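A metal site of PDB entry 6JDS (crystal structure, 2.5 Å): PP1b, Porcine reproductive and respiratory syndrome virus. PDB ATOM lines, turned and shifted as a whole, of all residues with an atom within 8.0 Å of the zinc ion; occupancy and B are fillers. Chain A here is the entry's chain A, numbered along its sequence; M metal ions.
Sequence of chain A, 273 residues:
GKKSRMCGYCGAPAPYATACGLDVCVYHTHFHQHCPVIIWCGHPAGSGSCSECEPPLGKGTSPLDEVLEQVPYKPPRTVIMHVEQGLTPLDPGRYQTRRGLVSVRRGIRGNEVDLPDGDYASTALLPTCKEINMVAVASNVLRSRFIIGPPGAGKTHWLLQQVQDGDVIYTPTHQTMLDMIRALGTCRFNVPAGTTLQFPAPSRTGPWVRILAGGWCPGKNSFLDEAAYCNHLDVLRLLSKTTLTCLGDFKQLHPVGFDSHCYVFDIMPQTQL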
ATOM      1  N   TYR A   9      19.424   7.705  13.868  1.00  0.00           N
ATOM      2  CA  TYR A   9      20.645   7.151  14.437  1.00  0.00           C
ATOM      3  C   TYR A   9      21.674   6.813  13.346  1.00  0.00           C
ATOM      4  O   TYR A   9      22.790   7.315  13.367  1.00  0.00           O
ATOM      5  CB  TYR A   9      20.353   5.881  15.231  1.00  0.00           C
ATOM      6  CG  TYR A   9      19.609   6.089  16.537  1.00  0.00           C
ATOM      7  CD1 TYR A   9      20.241   6.665  17.633  1.00  0.00           C
ATOM      8  CD2 TYR A   9      18.277   5.676  16.676  1.00  0.00           C
ATOM      9  CE1 TYR A   9      19.566   6.837  18.832  1.00  0.00           C
ATOM     10  CE2 TYR A   9      17.608   5.853  17.870  1.00  0.00           C
ATOM     11  CZ  TYR A   9      18.252   6.434  18.948  1.00  0.00           C
ATOM     12  OH  TYR A   9      17.582   6.611  20.141  1.00  0.00           O
ATOM     13  N   ALA A  17       8.784   5.576  13.649  1.00  0.00           N
ATOM     14  CA  ALA A  17       9.176   6.780  14.369  1.00  0.00           C
ATOM     15  C   ALA A  17       8.915   6.632  15.855  1.00  0.00           C
ATOM     16  O   ALA A  17       8.050   5.863  16.285  1.00  0.00           O
ATOM     17  CB  ALA A  17       8.425   7.985  13.827  1.00  0.00           C
ATOM     18  N   THR A  18       9.678   7.375  16.654  1.00  0.00           N
ATOM     19  CA  THR A  18       9.507   7.387  18.097  1.00  0.00           C
ATOM     20  C   THR A  18       8.344   8.306  18.413  1.00  0.00           C
ATOM     21  O   THR A  18       7.956   9.139  17.582  1.00  0.00           O
ATOM     22  CB  THR A  18      10.757   7.895  18.827  1.00  0.00           C
ATOM     23  OG1 THR A  18      11.027   9.248  18.435  1.00  0.00           O
ATOM     24  CG2 THR A  18      11.960   7.020  18.509  1.00  0.00           C
ATOM     25  N   ALA A  19       7.798   8.169  19.618  1.00  0.00           N
ATOM     26  CA  ALA A  19       6.747   9.064  20.086  1.00  0.00           C
ATOM     27  C   ALA A  19       7.245  10.513  20.166  1.00  0.00           C
ATOM     28  O   ALA A  19       6.451  11.453  20.061  1.00  0.00           O
ATOM     29  CB  ALA A  19       6.220   8.608  21.436  1.00  0.00           C
ATOM     30  N   CYS A  20       8.555  10.690  20.354  1.00  0.00           N
ATOM     31  CA  CYS A  20       9.181  12.010  20.478  1.00  0.00           C
ATOM     32  C   CYS A  20       9.701  12.603  19.152  1.00  0.00           C
ATOM     33  O   CYS A  20      10.364  13.638  19.169  1.00  0.00           O
ATOM     34  CB  CYS A  20      10.309  11.937  21.507  1.00  0.00           C
ATOM     35  SG  CYS A  20      11.774  11.022  20.967  1.00  0.00           S
ATOM     36  N   GLY A  21       9.414  11.948  18.028  1.00  0.00           N
ATOM     37  CA  GLY A  21       9.656  12.541  16.705  1.00  0.00           C
ATOM     38  C   GLY A  21      10.901  12.109  15.933  1.00  0.00           C
ATOM     39  O   GLY A  21      11.184  12.675  14.878  1.00  0.00           O
ATOM     40  N   LEU A  22      11.626  11.115  16.446  1.00  0.00           N
ATOM     41  CA  LEU A  22      12.809  10.600  15.755  1.00  0.00           C
ATOM     42  C   LEU A  22      12.431   9.449  14.836  1.00  0.00           C
ATOM     43  O   LEU A  22      11.742   8.519  15.255  1.00  0.00           O
ATOM     44  CB  LEU A  22      13.850  10.109  16.767  1.00  0.00           C
ATOM     45  CG  LEU A  22      15.238   9.771  16.228  1.00  0.00           C
ATOM     46  CD1 LEU A  22      16.050  11.035  15.958  1.00  0.00           C
ATOM     47  CD2 LEU A  22      15.996   8.864  17.189  1.00  0.00           C
ATOM     48  N   HIS A  32      15.558   2.493  21.875  1.00  0.00           N
ATOM     49  CA  HIS A  32      15.112   3.830  22.230  1.00  0.00           C
ATOM     50  C   HIS A  32      14.299   3.779  23.519  1.00  0.00           C
ATOM     51  O   HIS A  32      13.070   3.745  23.493  1.00  0.00           O
ATOM     52  CB  HIS A  32      14.295   4.440  21.083  1.00  0.00           C
ATOM     53  CG  HIS A  32      14.045   5.897  21.235  1.00  0.00           C
ATOM     54  ND1 HIS A  32      14.985   6.854  20.900  1.00  0.00           N
ATOM     55  CD2 HIS A  32      12.964   6.578  21.685  1.00  0.00           C
ATOM     56  CE1 HIS A  32      14.492   8.055  21.138  1.00  0.00           C
ATOM     57  NE2 HIS A  32      13.267   7.915  21.619  1.00  0.00           N
ATOM     58  N   GLN A  33      15.011   3.781  24.638  1.00  0.00           N
ATOM     59  CA  GLN A  33      14.422   3.656  25.971  1.00  0.00           C
ATOM     60  C   GLN A  33      13.572   4.878  26.345  1.00  0.00           C
ATOM     61  O   GLN A  33      12.640   4.760  27.130  1.00  0.00           O
ATOM     62  CB  GLN A  33      15.517   3.484  27.025  1.00  0.00           C
ATOM     63  CG  GLN A  33      16.375   2.226  26.875  1.00  0.00           C
ATOM     64  CD  GLN A  33      15.753   0.976  27.491  1.00  0.00           C
ATOM     65  OE1 GLN A  33      15.919  -0.127  26.961  1.00  0.00           O
ATOM     66  NE2 GLN A  33      15.046   1.145  28.599  1.00  0.00           N
ATOM     67  N   HIS A  34      13.923   6.043  25.794  1.00  0.00           N
ATOM     68  CA  HIS A  34      13.288   7.310  26.143  1.00  0.00           C
ATOM     69  C   HIS A  34      11.761   7.292  26.077  1.00  0.00           C
ATOM     70  O   HIS A  34      11.093   7.773  26.989  1.00  0.00           O
ATOM     71  CB  HIS A  34      13.843   8.426  25.245  1.00  0.00           C
ATOM     72  CG  HIS A  34      13.125   9.732  25.398  1.00  0.00           C
ATOM     73  ND1 HIS A  34      12.497  10.352  24.341  1.00  0.00           N
ATOM     74  CD2 HIS A  34      12.917  10.530  26.471  1.00  0.00           C
ATOM     75  CE1 HIS A  34      11.951  11.476  24.748  1.00  0.00           C
ATOM     76  NE2 HIS A  34      12.189  11.611  26.042  1.00  0.00           N
ATOM     77  N   CYS A  35      11.213   6.742  24.992  1.00  0.00           N
ATOM     78  CA  CYS A  35       9.763   6.788  24.769  1.00  0.00           C
ATOM     79  C   CYS A  35       9.312   5.622  23.880  1.00  0.00           C
ATOM     80  O   CYS A  35      10.154   4.963  23.246  1.00  0.00           O
ATOM     81  CB  CYS A  35       9.376   8.123  24.128  1.00  0.00           C
ATOM     82  SG  CYS A  35       9.814   8.272  22.386  1.00  0.00           S
ATOM     83  N   PRO A  36       7.988   5.354  23.817  1.00  0.00           N
ATOM     84  CA  PRO A  36       7.489   4.225  23.020  1.00  0.00           C
ATOM     85  C   PRO A  36       7.751   4.342  21.522  1.00  0.00           C
ATOM     86  O   PRO A  36       7.785   5.446  20.977  1.00  0.00           O
ATOM     87  CB  PRO A  36       5.976   4.249  23.283  1.00  0.00           C
ATOM     88  CG  PRO A  36       5.808   5.016  24.546  1.00  0.00           C
ATOM     89  CD  PRO A  36       6.904   6.038  24.537  1.00  0.00           C
ATOM     90  N   VAL A  37       7.942   3.187  20.876  1.00  0.00           N
ATOM     91  CA  VAL A  37       8.089   3.108  19.428  1.00  0.00           C
ATOM     92  C   VAL A  37       7.102   2.071  18.913  1.00  0.00           C
ATOM     93  O   VAL A  37       7.260   0.878  19.162  1.00  0.00           O
ATOM     94  CB  VAL A  37       9.526   2.710  19.025  1.00  0.00           C
ATOM     95  CG1 VAL A  37       9.662   2.662  17.508  1.00  0.00           C
ATOM     96  CG2 VAL A  37      10.536   3.666  19.627  1.00  0.00           C
ATOM     97  N   ASP A  65      20.864   9.462  23.083  1.00  0.00           N
ATOM     98  CA  ASP A  65      20.195   8.725  24.154  1.00  0.00           C
ATOM     99  C   ASP A  65      20.586   9.257  25.536  1.00  0.00           C
ATOM    100  O   ASP A  65      19.746   9.324  26.431  1.00  0.00           O
ATOM    101  CB  ASP A  65      20.491   7.220  24.057  1.00  0.00           C
ATOM    102  CG  ASP A  65      19.988   6.613  22.764  1.00  0.00           C
ATOM    103  OD1 ASP A  65      18.774   6.730  22.476  1.00  0.00           O
ATOM    104  OD2 ASP A  65      20.792   6.013  22.022  1.00  0.00           O
ATOM    105  N   LEU A  68      18.671  12.461  26.015  1.00  0.00           N
ATOM    106  CA  LEU A  68      17.261  12.174  26.287  1.00  0.00           C
ATOM    107  C   LEU A  68      16.974  11.664  27.700  1.00  0.00           C
ATOM    108  O   LEU A  68      15.834  11.679  28.142  1.00  0.00           O
ATOM    109  CB  LEU A  68      16.699  11.201  25.240  1.00  0.00           C
ATOM    110  CG  LEU A  68      16.475  11.811  23.857  1.00  0.00           C
ATOM    111  CD1 LEU A  68      16.208  10.724  22.818  1.00  0.00           C
ATOM    112  CD2 LEU A  68      15.354  12.831  23.874  1.00  0.00           C
ATOM    113  N   VAL A  71      15.504  14.465  29.510  1.00  0.00           N
ATOM    114  CA  VAL A  71      14.273  14.989  28.900  1.00  0.00           C
ATOM    115  C   VAL A  71      13.154  13.955  29.016  1.00  0.00           C
ATOM    116  O   VAL A  71      12.953  13.153  28.105  1.00  0.00           O
ATOM    117  CB  VAL A  71      14.504  15.362  27.412  1.00  0.00           C
ATOM    118  CG1 VAL A  71      13.244  15.996  26.812  1.00  0.00           C
ATOM    119  CG2 VAL A  71      15.698  16.288  27.269  1.00  0.00           C
ATOM    120  N   PRO A  72      12.426  13.962  30.152  1.00  0.00           N
ATOM    121  CA  PRO A  72      11.377  12.948  30.382  1.00  0.00           C
ATOM    122  C   PRO A  72      10.237  13.016  29.371  1.00  0.00           C
ATOM    123  O   PRO A  72       9.726  14.099  29.092  1.00  0.00           O
ATOM    124  CB  PRO A  72      10.871  13.283  31.789  1.00  0.00           C
ATOM    125  CG  PRO A  72      11.955  14.075  32.430  1.00  0.00           C
ATOM    126  CD  PRO A  72      12.572  14.854  31.309  1.00  0.00           C
ATOM    127  N   TYR A  73       9.857  11.860  28.838  1.00  0.00           N
ATOM    128  CA  TYR A  73       8.775  11.780  27.866  1.00  0.00           C
ATOM    129  C   TYR A  73       7.420  12.053  28.517  1.00  0.00           C
ATOM    130  O   TYR A  73       7.041  11.374  29.478  1.00  0.00           O
ATOM    131  CB  TYR A  73       8.762  10.409  27.172  1.00  0.00           C
ATOM    132  CG  TYR A  73       7.556  10.205  26.279  1.00  0.00           C
ATOM    133  CD1 TYR A  73       7.344  11.019  25.171  1.00  0.00           C
ATOM    134  CD2 TYR A  73       6.632   9.201  26.548  1.00  0.00           C
ATOM    135  CE1 TYR A  73       6.244  10.846  24.354  1.00  0.00           C
ATOM    136  CE2 TYR A  73       5.527   9.022  25.737  1.00  0.00           C
ATOM    137  CZ  TYR A  73       5.337   9.839  24.638  1.00  0.00           C
ATOM    138  OH  TYR A  73       4.240   9.655  23.830  1.00  0.00           O
ATOM    139  N   LEU A 126       5.751  14.246  19.343  1.00  0.00           N
ATOM    140  CA  LEU A 126       6.326  15.448  19.919  1.00  0.00           C
ATOM    141  C   LEU A 126       7.451  15.957  19.006  1.00  0.00           C
ATOM    142  O   LEU A 126       7.990  15.188  18.217  1.00  0.00           O
ATOM    143  CB  LEU A 126       6.863  15.178  21.325  1.00  0.00           C
ATOM    144  CG  LEU A 126       5.854  14.602  22.333  1.00  0.00           C
ATOM    145  CD1 LEU A 126       6.516  14.389  23.681  1.00  0.00           C
ATOM    146  CD2 LEU A 126       4.636  15.502  22.480  1.00  0.00           C
ATOM    147  N   THR A 128      10.342  16.897  20.042  1.00  0.00           N
ATOM    148  CA  THR A 128      11.587  16.693  20.777  1.00  0.00           C
ATOM    149  C   THR A 128      12.786  16.332  19.902  1.00  0.00           C
ATOM    150  O   THR A 128      13.822  16.970  19.993  1.00  0.00           O
ATOM    151  CB  THR A 128      11.415  15.595  21.842  1.00  0.00           C
ATOM    152  OG1 THR A 128      10.193  15.813  22.565  1.00  0.00           O
ATOM    153  CG2 THR A 128      12.577  15.567  22.828  1.00  0.00           C
ATOM    154  N   CYS A 129      12.637  15.309  19.057  1.00  0.00           N
ATOM    155  CA  CYS A 129      13.723  14.846  18.187  1.00  0.00           C
ATOM    156  C   CYS A 129      13.403  15.031  16.698  1.00  0.00           C
ATOM    157  O   CYS A 129      13.898  14.292  15.855  1.00  0.00           O
ATOM    158  CB  CYS A 129      14.049  13.375  18.480  1.00  0.00           C
ATOM    159  SG  CYS A 129      14.817  13.109  20.088  1.00  0.00           S
HETATM  160 ZN    ZN M   1      11.784   9.369  22.508  1.00  0.00          ZN
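ND1 of His 34 binds the zinc ion (2.2 Å).
SG of Cys 35 is bound to the zinc ion.
The zinc ion is bound by NE2 of His 32, 2.3 Å away.
The zinc ion is bound by SG of Cys 20 (2.3 Å).
The zinc ion has four donor atoms within binding distance.
The side-chain hydroxyl (OH) of Tyr 9 sits at hydrogen-bond distance from a ring nitrogen (ND1) of His 32.
The backbone NH (N) of Cys 20 lies close to the side-chain hydroxyl (OG1) of Thr 18 (3.4 Å).
O of Cys 20 is in hydrogen-bond range of N of Thr 128.
The backbone NH of Ala 19 lies close to the side-chain sulfur of Cys 35 (3.4 Å).
NE2 of His 34 lies within hydrogen-bond range of O of Val 71, 2.7 Å away.
The backbone carbonyl oxygen of Cys 20 sits at hydrogen-bond distance from the backbone NH of Cys 129 (2.8 Å).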
